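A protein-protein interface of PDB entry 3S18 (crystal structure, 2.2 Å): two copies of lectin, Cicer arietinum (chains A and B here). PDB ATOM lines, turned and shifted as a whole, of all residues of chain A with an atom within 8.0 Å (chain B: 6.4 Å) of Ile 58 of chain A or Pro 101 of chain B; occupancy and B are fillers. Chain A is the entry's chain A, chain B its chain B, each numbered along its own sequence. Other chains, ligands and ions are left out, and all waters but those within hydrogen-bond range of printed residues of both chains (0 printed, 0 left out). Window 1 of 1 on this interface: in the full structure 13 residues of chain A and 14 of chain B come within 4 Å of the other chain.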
ATOM      1  N   ASP A  24     -33.759   8.698   7.737  1.00  0.00           N
ATOM      2  CA  ASP A  24     -32.451   8.645   7.097  1.00  0.00           C
ATOM      3  C   ASP A  24     -32.461   7.745   5.853  1.00  0.00           C
ATOM      4  O   ASP A  24     -31.413   7.362   5.327  1.00  0.00           O
ATOM      5  CB  ASP A  24     -31.375   8.232   8.102  1.00  0.00           C
ATOM      6  CG  ASP A  24     -31.669   6.896   8.775  1.00  0.00           C
ATOM      7  OD1 ASP A  24     -32.752   6.301   8.548  1.00  0.00           O
ATOM      8  OD2 ASP A  24     -30.801   6.446   9.542  1.00  0.00           O
ATOM      9  N   VAL A  47     -29.931   6.653   2.825  1.00  0.00           N
ATOM     10  CA  VAL A  47     -29.388   7.643   1.908  1.00  0.00           C
ATOM     11  C   VAL A  47     -27.906   7.351   1.679  1.00  0.00           C
ATOM     12  O   VAL A  47     -27.411   7.423   0.546  1.00  0.00           O
ATOM     13  CB  VAL A  47     -29.620   9.109   2.413  1.00  0.00           C
ATOM     14  CG1 VAL A  47     -28.823  10.133   1.579  1.00  0.00           C
ATOM     15  CG2 VAL A  47     -31.116   9.458   2.392  1.00  0.00           C
ATOM     16  N   ARG A  48     -27.209   6.979   2.748  1.00  0.00           N
ATOM     17  CA  ARG A  48     -25.773   6.733   2.652  1.00  0.00           C
ATOM     18  C   ARG A  48     -25.434   5.483   1.826  1.00  0.00           C
ATOM     19  O   ARG A  48     -24.331   5.381   1.313  1.00  0.00           O
ATOM     20  CB  ARG A  48     -25.133   6.668   4.036  1.00  0.00           C
ATOM     21  CG  ARG A  48     -25.458   5.422   4.823  1.00  0.00           C
ATOM     22  CD  ARG A  48     -24.870   5.502   6.215  1.00  0.00           C
ATOM     23  NE  ARG A  48     -25.583   4.618   7.134  1.00  0.00           N
ATOM     24  CZ  ARG A  48     -26.573   5.001   7.935  1.00  0.00           C
ATOM     25  NH1 ARG A  48     -26.974   6.271   7.960  1.00  0.00           N
ATOM     26  NH2 ARG A  48     -27.159   4.106   8.725  1.00  0.00           N
ATOM     27  N   LEU A  54     -22.837  10.954  -0.736  1.00  0.00           N
ATOM     28  CA  LEU A  54     -23.320  11.465   0.562  1.00  0.00           C
ATOM     29  C   LEU A  54     -22.940  10.633   1.802  1.00  0.00           C
ATOM     30  O   LEU A  54     -23.310  10.987   2.933  1.00  0.00           O
ATOM     31  CB  LEU A  54     -24.839  11.683   0.516  1.00  0.00           C
ATOM     32  CG  LEU A  54     -25.341  12.589  -0.617  1.00  0.00           C
ATOM     33  CD1 LEU A  54     -26.865  12.607  -0.666  1.00  0.00           C
ATOM     34  CD2 LEU A  54     -24.798  14.003  -0.460  1.00  0.00           C
ATOM     35  N   ALA A  55     -22.171   9.558   1.597  1.00  0.00           N
ATOM     36  CA  ALA A  55     -21.933   8.560   2.646  1.00  0.00           C
ATOM     37  C   ALA A  55     -21.304   9.137   3.905  1.00  0.00           C
ATOM     38  O   ALA A  55     -21.748   8.842   5.017  1.00  0.00           O
ATOM     39  CB  ALA A  55     -21.087   7.380   2.116  1.00  0.00           C
ATOM     40  N   LYS A  56     -20.279   9.952   3.746  1.00  0.00           N
ATOM     41  CA  LYS A  56     -19.594  10.489   4.915  1.00  0.00           C
ATOM     42  C   LYS A  56     -19.933  11.968   5.140  1.00  0.00           C
ATOM     43  O   LYS A  56     -19.057  12.799   5.354  1.00  0.00           O
ATOM     44  CB  LYS A  56     -18.076  10.269   4.784  1.00  0.00           C
ATOM     45  CG  LYS A  56     -17.623   8.791   4.660  1.00  0.00           C
ATOM     46  CD  LYS A  56     -18.388   7.866   5.573  1.00  0.00           C
ATOM     47  CE  LYS A  56     -18.147   8.186   7.033  1.00  0.00           C
ATOM     48  NZ  LYS A  56     -18.993   7.331   7.937  1.00  0.00           N
ATOM     49  N   THR A  57     -21.221  12.285   5.088  1.00  0.00           N
ATOM     50  CA  THR A  57     -21.685  13.650   5.236  1.00  0.00           C
ATOM     51  C   THR A  57     -22.825  13.620   6.234  1.00  0.00           C
ATOM     52  O   THR A  57     -23.336  12.540   6.562  1.00  0.00           O
ATOM     53  CB  THR A  57     -22.161  14.244   3.872  1.00  0.00           C
ATOM     54  OG1 THR A  57     -23.380  13.611   3.457  1.00  0.00           O
ATOM     55  CG2 THR A  57     -21.071  14.067   2.778  1.00  0.00           C
ATOM     56  N   ILE A  58     -23.208  14.790   6.742  1.00  0.00           N
ATOM     57  CA  ILE A  58     -24.360  14.888   7.638  1.00  0.00           C
ATOM     58  C   ILE A  58     -25.661  14.370   6.981  1.00  0.00           C
ATOM     59  O   ILE A  58     -26.533  13.830   7.675  1.00  0.00           O
ATOM     60  CB  ILE A  58     -24.545  16.319   8.188  1.00  0.00           C
ATOM     61  CG1 ILE A  58     -24.872  17.302   7.051  1.00  0.00           C
ATOM     62  CG2 ILE A  58     -23.317  16.732   9.023  1.00  0.00           C
ATOM     63  CD1 ILE A  58     -25.001  18.734   7.453  1.00  0.00           C
ATOM     64  N   PHE A  59     -25.777  14.527   5.659  1.00  0.00           N
ATOM     65  CA  PHE A  59     -26.918  13.998   4.897  1.00  0.00           C
ATOM     66  C   PHE A  59     -26.949  12.488   4.933  1.00  0.00           C
ATOM     67  O   PHE A  59     -28.008  11.908   5.044  1.00  0.00           O
ATOM     68  CB  PHE A  59     -26.924  14.483   3.437  1.00  0.00           C
ATOM     69  CG  PHE A  59     -26.716  15.957   3.300  1.00  0.00           C
ATOM     70  CD1 PHE A  59     -27.752  16.846   3.570  1.00  0.00           C
ATOM     71  CD2 PHE A  59     -25.473  16.457   2.930  1.00  0.00           C
ATOM     72  CE1 PHE A  59     -27.550  18.220   3.472  1.00  0.00           C
ATOM     73  CE2 PHE A  59     -25.252  17.826   2.833  1.00  0.00           C
ATOM     74  CZ  PHE A  59     -26.307  18.717   3.098  1.00  0.00           C
ATOM     75  N   GLY A  60     -25.785  11.847   4.853  1.00  0.00           N
ATOM     76  CA  GLY A  60     -25.714  10.391   4.936  1.00  0.00           C
ATOM     77  C   GLY A  60     -26.061   9.881   6.319  1.00  0.00           C
ATOM     78  O   GLY A  60     -26.657   8.800   6.472  1.00  0.00           O
ATOM     79  N   THR A  61     -25.679  10.651   7.341  1.00  0.00           N
ATOM     80  CA  THR A  61     -25.971  10.269   8.719  1.00  0.00           C
ATOM     81  C   THR A  61     -27.436  10.512   9.110  1.00  0.00           C
ATOM     82  O   THR A  61     -28.061   9.649   9.708  1.00  0.00           O
ATOM     83  CB  THR A  61     -25.073  11.017   9.693  1.00  0.00           C
ATOM     84  OG1 THR A  61     -23.719  10.860   9.279  1.00  0.00           O
ATOM     85  CG2 THR A  61     -25.260  10.505  11.148  1.00  0.00           C
ATOM     86  N   TYR A  62     -27.975  11.683   8.799  1.00  0.00           N
ATOM     87  CA  TYR A  62     -29.288  12.060   9.328  1.00  0.00           C
ATOM     88  C   TYR A  62     -30.403  12.119   8.288  1.00  0.00           C
ATOM     89  O   TYR A  62     -31.572  12.171   8.652  1.00  0.00           O
ATOM     90  CB  TYR A  62     -29.200  13.375  10.116  1.00  0.00           C
ATOM     91  CG  TYR A  62     -28.314  13.255  11.341  1.00  0.00           C
ATOM     92  CD1 TYR A  62     -28.739  12.535  12.465  1.00  0.00           C
ATOM     93  CD2 TYR A  62     -27.054  13.848  11.375  1.00  0.00           C
ATOM     94  CE1 TYR A  62     -27.923  12.414  13.599  1.00  0.00           C
ATOM     95  CE2 TYR A  62     -26.227  13.731  12.515  1.00  0.00           C
ATOM     96  CZ  TYR A  62     -26.671  13.001  13.603  1.00  0.00           C
ATOM     97  OH  TYR A  62     -25.882  12.878  14.706  1.00  0.00           O
ATOM     98  N   GLY A  63     -30.043  12.086   7.004  1.00  0.00           N
ATOM     99  CA  GLY A  63     -31.050  12.164   5.946  1.00  0.00           C
ATOM    100  C   GLY A  63     -31.266  13.595   5.480  1.00  0.00           C
ATOM    101  O   GLY A  63     -30.453  14.479   5.771  1.00  0.00           O
ATOM    102  N   ILE A  64     -32.373  13.812   4.775  1.00  0.00           N
ATOM    103  CA  ILE A  64     -32.626  15.025   4.019  1.00  0.00           C
ATOM    104  C   ILE A  64     -34.003  15.573   4.401  1.00  0.00           C
ATOM    105  O   ILE A  64     -35.016  14.896   4.226  1.00  0.00           O
ATOM    106  CB  ILE A  64     -32.550  14.709   2.497  1.00  0.00           C
ATOM    107  CG1 ILE A  64     -31.088  14.466   2.095  1.00  0.00           C
ATOM    108  CG2 ILE A  64     -33.183  15.824   1.654  1.00  0.00           C
ATOM    109  CD1 ILE A  64     -30.918  13.543   0.854  1.00  0.00           C
ATOM    110  N   ILE A  77     -30.487  19.783  -1.833  1.00  0.00           N
ATOM    111  CA  ILE A  77     -30.912  18.983  -0.695  1.00  0.00           C
ATOM    112  C   ILE A  77     -30.533  19.728   0.587  1.00  0.00           C
ATOM    113  O   ILE A  77     -29.588  20.508   0.579  1.00  0.00           O
ATOM    114  CB  ILE A  77     -30.299  17.554  -0.726  1.00  0.00           C
ATOM    115  CG1 ILE A  77     -28.759  17.597  -0.678  1.00  0.00           C
ATOM    116  CG2 ILE A  77     -30.798  16.791  -1.972  1.00  0.00           C
ATOM    117  CD1 ILE A  77     -28.116  16.258  -0.352  1.00  0.00           C
ATOM    118  N   PHE A  78     -31.289  19.502   1.664  1.00  0.00           N
ATOM    119  CA  PHE A  78     -31.118  20.244   2.910  1.00  0.00           C
ATOM    120  C   PHE A  78     -31.117  19.340   4.121  1.00  0.00           C
ATOM    121  O   PHE A  78     -31.716  18.278   4.104  1.00  0.00           O
ATOM    122  CB  PHE A  78     -32.256  21.232   3.110  1.00  0.00           C
ATOM    123  CG  PHE A  78     -32.334  22.316   2.071  1.00  0.00           C
ATOM    124  CD1 PHE A  78     -31.818  23.583   2.346  1.00  0.00           C
ATOM    125  CD2 PHE A  78     -32.970  22.087   0.850  1.00  0.00           C
ATOM    126  CE1 PHE A  78     -31.908  24.624   1.404  1.00  0.00           C
ATOM    127  CE2 PHE A  78     -33.071  23.125  -0.121  1.00  0.00           C
ATOM    128  CZ  PHE A  78     -32.532  24.399   0.173  1.00  0.00           C
ATOM    129  N   TYR A  79     -30.454  19.796   5.182  1.00  0.00           N
ATOM    130  CA  TYR A  79     -30.629  19.219   6.495  1.00  0.00           C
ATOM    131  C   TYR A  79     -30.312  20.302   7.500  1.00  0.00           C
ATOM    132  O   TYR A  79     -29.180  20.783   7.539  1.00  0.00           O
ATOM    133  CB  TYR A  79     -29.748  17.974   6.720  1.00  0.00           C
ATOM    134  CG  TYR A  79     -29.960  17.408   8.094  1.00  0.00           C
ATOM    135  CD1 TYR A  79     -31.069  16.613   8.379  1.00  0.00           C
ATOM    136  CD2 TYR A  79     -29.076  17.711   9.131  1.00  0.00           C
ATOM    137  CE1 TYR A  79     -31.285  16.128   9.650  1.00  0.00           C
ATOM    138  CE2 TYR A  79     -29.276  17.231  10.382  1.00  0.00           C
ATOM    139  CZ  TYR A  79     -30.381  16.444  10.645  1.00  0.00           C
ATOM    140  OH  TYR A  79     -30.555  15.971  11.928  1.00  0.00           O
ATOM    141  N   GLU A  80     -31.312  20.681   8.298  1.00  0.00           N
ATOM    142  CA  GLU A  80     -31.211  21.826   9.222  1.00  0.00           C
ATOM    143  C   GLU A  80     -30.679  23.058   8.478  1.00  0.00           C
ATOM    144  O   GLU A  80     -31.166  23.358   7.384  1.00  0.00           O
ATOM    145  CB  GLU A  80     -30.424  21.448  10.490  1.00  0.00           C
ATOM    146  CG  GLU A  80     -31.118  20.279  11.257  1.00  0.00           C
ATOM    147  CD  GLU A  80     -30.445  19.889  12.560  1.00  0.00           C
ATOM    148  OE1 GLU A  80     -29.339  20.397  12.872  1.00  0.00           O
ATOM    149  OE2 GLU A  80     -31.045  19.065  13.285  1.00  0.00           O
ATOM    150  N   ASN A  81     -29.686  23.751   9.019  1.00  0.00           N
ATOM    151  CA  ASN A  81     -29.202  24.958   8.350  1.00  0.00           C
ATOM    152  C   ASN A  81     -28.229  24.740   7.178  1.00  0.00           C
ATOM    153  O   ASN A  81     -27.668  25.699   6.684  1.00  0.00           O
ATOM    154  CB  ASN A  81     -28.668  26.011   9.367  1.00  0.00           C
ATOM    155  CG  ASN A  81     -27.408  25.572  10.072  1.00  0.00           C
ATOM    156  OD1 ASN A  81     -26.949  24.462   9.860  1.00  0.00           O
ATOM    157  ND2 ASN A  81     -26.836  26.442  10.930  1.00  0.00           N
ATOM    158  N   PHE A  82     -28.041  23.494   6.743  1.00  0.00           N
ATOM    159  CA  PHE A  82     -27.056  23.168   5.697  1.00  0.00           C
ATOM    160  C   PHE A  82     -27.715  22.688   4.426  1.00  0.00           C
ATOM    161  O   PHE A  82     -28.820  22.132   4.470  1.00  0.00           O
ATOM    162  CB  PHE A  82     -26.056  22.107   6.162  1.00  0.00           C
ATOM    163  CG  PHE A  82     -25.192  22.555   7.295  1.00  0.00           C
ATOM    164  CD1 PHE A  82     -24.067  23.342   7.063  1.00  0.00           C
ATOM    165  CD2 PHE A  82     -25.500  22.197   8.603  1.00  0.00           C
ATOM    166  CE1 PHE A  82     -23.266  23.769   8.122  1.00  0.00           C
ATOM    167  CE2 PHE A  82     -24.702  22.622   9.674  1.00  0.00           C
ATOM    168  CZ  PHE A  82     -23.590  23.406   9.431  1.00  0.00           C
ATOM    169  N   CYS A  83     -27.045  22.910   3.289  1.00  0.00           N
ATOM    170  CA  CYS A  83     -27.568  22.401   2.008  1.00  0.00           C
ATOM    171  C   CYS A  83     -26.460  22.105   1.028  1.00  0.00           C
ATOM    172  O   CYS A  83     -25.309  22.485   1.244  1.00  0.00           O
ATOM    173  CB  CYS A  83     -28.567  23.381   1.380  1.00  0.00           C
ATOM    174  SG  CYS A  83     -27.851  24.982   1.032  1.00  0.00           S
ATOM    175  N   PRO A 101     -21.027  21.165   0.698  1.00  0.00           N
ATOM    176  CA  PRO A 101     -22.162  21.699   1.427  1.00  0.00           C
ATOM    177  C   PRO A 101     -21.878  23.078   2.054  1.00  0.00           C
ATOM    178  O   PRO A 101     -20.746  23.370   2.457  1.00  0.00           O
ATOM    179  CB  PRO A 101     -22.414  20.637   2.495  1.00  0.00           C
ATOM    180  CG  PRO A 101     -21.088  20.006   2.715  1.00  0.00           C
ATOM    181  CD  PRO A 101     -20.279  20.160   1.472  1.00  0.00           C
ATOM    182  N   LYS A 102     -22.917  23.909   2.089  1.00  0.00           N
ATOM    183  CA  LYS A 102     -22.870  25.257   2.650  1.00  0.00           C
ATOM    184  C   LYS A 102     -24.012  25.414   3.623  1.00  0.00           C
ATOM    185  O   LYS A 102     -25.035  24.733   3.490  1.00  0.00           O
ATOM    186  CB  LYS A 102     -23.106  26.305   1.555  1.00  0.00           C
ATOM    187  CG  LYS A 102     -21.964  26.492   0.586  1.00  0.00           C
ATOM    188  CD  LYS A 102     -22.090  27.837  -0.079  1.00  0.00           C
ATOM    189  CE  LYS A 102     -21.034  28.030  -1.144  1.00  0.00           C
ATOM    190  NZ  LYS A 102     -21.057  26.831  -2.020  1.00  0.00           N
ATOM    191  N   THR B  57     -17.446  17.861   2.859  1.00  0.00           N
ATOM    192  CA  THR B  57     -18.139  17.881   4.142  1.00  0.00           C
ATOM    193  C   THR B  57     -18.200  19.319   4.660  1.00  0.00           C
ATOM    194  O   THR B  57     -17.516  20.206   4.130  1.00  0.00           O
ATOM    195  CB  THR B  57     -17.378  17.077   5.230  1.00  0.00           C
ATOM    196  OG1 THR B  57     -16.161  17.762   5.560  1.00  0.00           O
ATOM    197  CG2 THR B  57     -17.078  15.645   4.777  1.00  0.00           C
ATOM    198  N   ILE B  58     -18.980  19.543   5.718  1.00  0.00           N
ATOM    199  CA  ILE B  58     -19.013  20.854   6.359  1.00  0.00           C
ATOM    200  C   ILE B  58     -17.624  21.255   6.907  1.00  0.00           C
ATOM    201  O   ILE B  58     -17.306  22.442   6.969  1.00  0.00           O
ATOM    202  CB  ILE B  58     -20.109  20.948   7.446  1.00  0.00           C
ATOM    203  CG1 ILE B  58     -19.822  19.961   8.597  1.00  0.00           C
ATOM    204  CG2 ILE B  58     -21.492  20.729   6.814  1.00  0.00           C
ATOM    205  CD1 ILE B  58     -20.833  19.965   9.720  1.00  0.00           C
ATOM    206  N   PHE B  59     -16.806  20.272   7.276  1.00  0.00           N
ATOM    207  CA  PHE B  59     -15.437  20.526   7.741  1.00  0.00           C
ATOM    208  C   PHE B  59     -14.541  21.076   6.638  1.00  0.00           C
ATOM    209  O   PHE B  59     -13.626  21.858   6.905  1.00  0.00           O
ATOM    210  CB  PHE B  59     -14.814  19.259   8.347  1.00  0.00           C
ATOM    211  CG  PHE B  59     -15.664  18.620   9.417  1.00  0.00           C
ATOM    212  CD1 PHE B  59     -15.833  19.235  10.647  1.00  0.00           C
ATOM    213  CD2 PHE B  59     -16.298  17.395   9.181  1.00  0.00           C
ATOM    214  CE1 PHE B  59     -16.616  18.643  11.639  1.00  0.00           C
ATOM    215  CE2 PHE B  59     -17.080  16.791  10.158  1.00  0.00           C
ATOM    216  CZ  PHE B  59     -17.245  17.421  11.396  1.00  0.00           C
ATOM    217  N   PHE B  82     -21.473  19.584  15.286  1.00  0.00           N
ATOM    218  CA  PHE B  82     -21.069  18.344  14.615  1.00  0.00           C
ATOM    219  C   PHE B  82     -19.620  17.956  14.887  1.00  0.00           C
ATOM    220  O   PHE B  82     -18.769  18.813  15.121  1.00  0.00           O
ATOM    221  CB  PHE B  82     -21.296  18.450  13.112  1.00  0.00           C
ATOM    222  CG  PHE B  82     -22.727  18.560  12.736  1.00  0.00           C
ATOM    223  CD1 PHE B  82     -23.530  17.425  12.663  1.00  0.00           C
ATOM    224  CD2 PHE B  82     -23.291  19.807  12.447  1.00  0.00           C
ATOM    225  CE1 PHE B  82     -24.894  17.533  12.309  1.00  0.00           C
ATOM    226  CE2 PHE B  82     -24.645  19.918  12.092  1.00  0.00           C
ATOM    227  CZ  PHE B  82     -25.446  18.778  12.042  1.00  0.00           C
ATOM    228  N   CYS B  83     -19.354  16.653  14.835  1.00  0.00           N
ATOM    229  CA  CYS B  83     -18.030  16.109  15.070  1.00  0.00           C
ATOM    230  C   CYS B  83     -17.803  14.809  14.284  1.00  0.00           C
ATOM    231  O   CYS B  83     -18.746  14.184  13.792  1.00  0.00           O
ATOM    232  CB  CYS B  83     -17.809  15.872  16.569  1.00  0.00           C
ATOM    233  SG  CYS B  83     -18.905  14.636  17.296  1.00  0.00           S
ATOM    234  N   ALA B  84     -16.545  14.415  14.152  1.00  0.00           N
ATOM    235  CA  ALA B  84     -16.199  13.211  13.431  1.00  0.00           C
ATOM    236  C   ALA B  84     -14.931  12.693  14.037  1.00  0.00           C
ATOM    237  O   ALA B  84     -14.145  13.463  14.595  1.00  0.00           O
ATOM    238  CB  ALA B  84     -15.970  13.510  11.926  1.00  0.00           C
ATOM    239  N   ILE B  97     -12.312   9.387   7.235  1.00  0.00           N
ATOM    240  CA  ILE B  97     -13.298   9.457   8.308  1.00  0.00           C
ATOM    241  C   ILE B  97     -13.552   8.046   8.835  1.00  0.00           C
ATOM    242  O   ILE B  97     -13.795   7.129   8.047  1.00  0.00           O
ATOM    243  CB  ILE B  97     -14.621  10.122   7.848  1.00  0.00           C
ATOM    244  CG1 ILE B  97     -14.340  11.523   7.288  1.00  0.00           C
ATOM    245  CG2 ILE B  97     -15.608  10.206   9.015  1.00  0.00           C
ATOM    246  CD1 ILE B  97     -15.494  12.118   6.454  1.00  0.00           C
ATOM    247  N   SER B  99     -15.693   7.627  11.958  1.00  0.00           N
ATOM    248  CA  SER B  99     -17.056   7.731  12.495  1.00  0.00           C
ATOM    249  C   SER B  99     -17.581   9.140  12.228  1.00  0.00           C
ATOM    250  O   SER B  99     -16.874  10.130  12.456  1.00  0.00           O
ATOM    251  CB  SER B  99     -17.071   7.491  14.011  1.00  0.00           C
ATOM    252  OG  SER B  99     -17.272   6.123  14.357  1.00  0.00           O
ATOM    253  N   GLY B 100     -18.820   9.221  11.749  1.00  0.00           N
ATOM    254  CA  GLY B 100     -19.505  10.490  11.572  1.00  0.00           C
ATOM    255  C   GLY B 100     -19.518  10.973  10.145  1.00  0.00           C
ATOM    256  O   GLY B 100     -19.267  10.185   9.220  1.00  0.00           O
ATOM    257  N   PRO B 101     -19.830  12.267   9.934  1.00  0.00           N
ATOM    258  CA  PRO B 101     -20.153  13.291  10.938  1.00  0.00           C
ATOM    259  C   PRO B 101     -21.408  12.929  11.735  1.00  0.00           C
ATOM    260  O   PRO B 101     -22.311  12.280  11.208  1.00  0.00           O
ATOM    261  CB  PRO B 101     -20.407  14.555  10.107  1.00  0.00           C
ATOM    262  CG  PRO B 101     -20.057  14.197   8.658  1.00  0.00           C
ATOM    263  CD  PRO B 101     -20.104  12.721   8.557  1.00  0.00           C
ATOM    264  N   LYS B 102     -21.431  13.321  13.001  1.00  0.00           N
ATOM    265  CA  LYS B 102     -22.549  13.074  13.897  1.00  0.00           C
ATOM    266  C   LYS B 102     -22.692  14.326  14.739  1.00  0.00           C
ATOM    267  O   LYS B 102     -21.706  15.057  14.946  1.00  0.00           O
ATOM    268  CB  LYS B 102     -22.223  11.917  14.854  1.00  0.00           C
ATOM    269  CG  LYS B 102     -22.612  10.510  14.382  1.00  0.00           C
ATOM    270  CD  LYS B 102     -22.279   9.472  15.474  1.00  0.00           C
ATOM    271  CE  LYS B 102     -23.191   8.248  15.446  1.00  0.00           C
ATOM    272  NZ  LYS B 102     -23.004   7.379  14.248  1.00  0.00           N
ATOM    273  N   LYS B 103     -23.892  14.554  15.263  1.00  0.00           N
ATOM    274  CA  LYS B 103     -24.076  15.585  16.268  1.00  0.00           C
ATOM    275  C   LYS B 103     -23.323  15.158  17.515  1.00  0.00           C
ATOM    276  O   LYS B 103     -23.174  13.950  17.789  1.00  0.00           O
ATOM    277  CB  LYS B 103     -25.563  15.806  16.586  1.00  0.00           C
ATOM    278  CG  LYS B 103     -26.369  16.289  15.368  1.00  0.00           C
ATOM    279  CD  LYS B 103     -27.862  16.298  15.636  1.00  0.00           C
ATOM    280  CE  LYS B 103     -28.590  17.173  14.623  1.00  0.00           C
ATOM    281  NZ  LYS B 103     -30.042  17.402  14.969  1.00  0.00           N
ATOM    282  N   MET B 107     -22.694  11.458  19.427  1.00  0.00           N
ATOM    283  CA  MET B 107     -21.369  10.925  19.689  1.00  0.00           C
ATOM    284  C   MET B 107     -21.094  10.828  21.193  1.00  0.00           C
ATOM    285  O   MET B 107     -20.459   9.880  21.647  1.00  0.00           O
ATOM    286  CB  MET B 107     -20.303  11.800  19.021  1.00  0.00           C
ATOM    287  CG  MET B 107     -18.904  11.190  19.027  1.00  0.00           C
ATOM    288  SD  MET B 107     -18.781   9.845  17.836  1.00  0.00           S
ATOM    289  CE  MET B 107     -18.396  10.764  16.349  1.00  0.00           C
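Of chain B, only Phe 82 and Pro 101 come within 4 Å of Ile 58 of chain A.
Pro 101 of chain B touches just these residues of chain A: Lys 56 (3.4 Å), Thr 57 (3.7 Å), Ile 58 (3.7 Å) and Thr 61 (2.8 Å).
Of the printed residues of chain B, Pro 101 of chain A touches Thr 57 and Ile 58.
Of the printed residues of chain B, Thr 61 of chain A touches Pro 101 (2.8 Å).
Asn 81 of chain A touches none of the printed residues of chain B.
The nearest residue of chain B that does not touch Ile 58 of chain A is Ile 58 of chain B (4.1 Å).
The nearest printed residue of chain B that does not touch Thr 61 of chain A is Lys 102 of chain B (4.2 Å).
The backbone carbonyl oxygen (O) of Leu 54 of chain A sits at hydrogen-bond distance from the side-chain hydroxyl (OG1) of Thr 57 of chain A.
OG1 of Thr 57 of chain A lies close to N of Phe 59 of chain A (3.4 Å).
OG1 of Thr 61 of chain A sits at hydrogen-bond distance from O of Thr 57 of chain A.
OE2 of Glu 80 of chain A sits at hydrogen-bond distance from OH of Tyr 79 of chain A, 3.4 Å away.
OG1 of Thr 57 of chain B lies within hydrogen-bond range of N of Phe 59 of chain B.
The backbone NH (N) of Cys 83 of chain B lies within hydrogen-bond range of the backbone carbonyl oxygen (O) of Lys 102 of chain B, 2.8 Å away.
Thr 57 of chain A touches Pro 101 of chain B, and with the chains exchanged Pro 101 of chain A touches Thr 57 of chain B.
Ile 58 of chain A touches Phe 82 of chain B, and with the chains exchanged Phe 82 of chain A touches Ile 58 of chain B.
Ile 58 of chain A touches Pro 101 of chain B, and with the chains exchanged Pro 101 of chain A touches Ile 58 of chain B.
Phe 82 of chain A touches its own counterpart, Phe 82 of chain B.
7 positions are printed for both chains.
Of the 16 pairs that touch across the chains among the printed residues, 7 have their exchanged pair printed and touching as well.
NZ of Lys 56 of chain A is in hydrogen-bond range of O of Gly 100 of chain B, at 3.1 Å.
The side-chain hydroxyl (OG1) of Thr 61 of chain A is in hydrogen-bond range of the backbone carbonyl oxygen (O) of Pro 101 of chain B, at 2.8 Å.
OH of Tyr 62 of chain A lies within hydrogen-bond range of N of Lys 103 of chain B (2.7 Å).
OH of Tyr 79 of chain A is in hydrogen-bond range of NZ of Lys 103 of chain B (3.4 Å).
NZ of Lys 103 of chain B is in salt-bridge range of OE2 of Glu 80 of chain A.
Printed residues of chain B that touch a printed residue of chain A: Thr 57, Ile 58, Phe 82, Ile 97, Gly 100, Pro 101, Lys 102 and Lys 103.
Of the 23 printed residues of chain A, 9 touch a printed residue of chain B.
Among the printed residues, Asp or Glu carboxylates within 4 Å of a Lys or Arg side-chain nitrogen of the other chain: Glu 80 of chain A with Lys 103 of chain B (2.6 Å).
Among the printed residues, merely in contact across the chains: Lys 56 of chain A with Pro 101 of chain B (3.4 Å), Tyr 62 of chain A with Lys 102 of chain B (3.4 Å), Lys 56 of chain A with Thr 57 of chain B (3.5 Å), Pro 101 of chain A with Thr 57 of chain B (3.5 Å), Lys 56 of chain A with Ile 97 of chain B (3.6 Å), Phe 82 of chain A with Phe 82 of chain B (3.6 Å), Thr 57 of chain A with Pro 101 of chain B (3.7 Å), Phe 82 of chain A with Ile 58 of chain B (3.7 Å), Pro 101 of chain A with Ile 58 of chain B (3.7 Å), Ile 58 of chain A with Phe 82 of chain B (3.7 Å) and Ile 58 of chain A with Pro 101 of chain B (3.7 Å).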
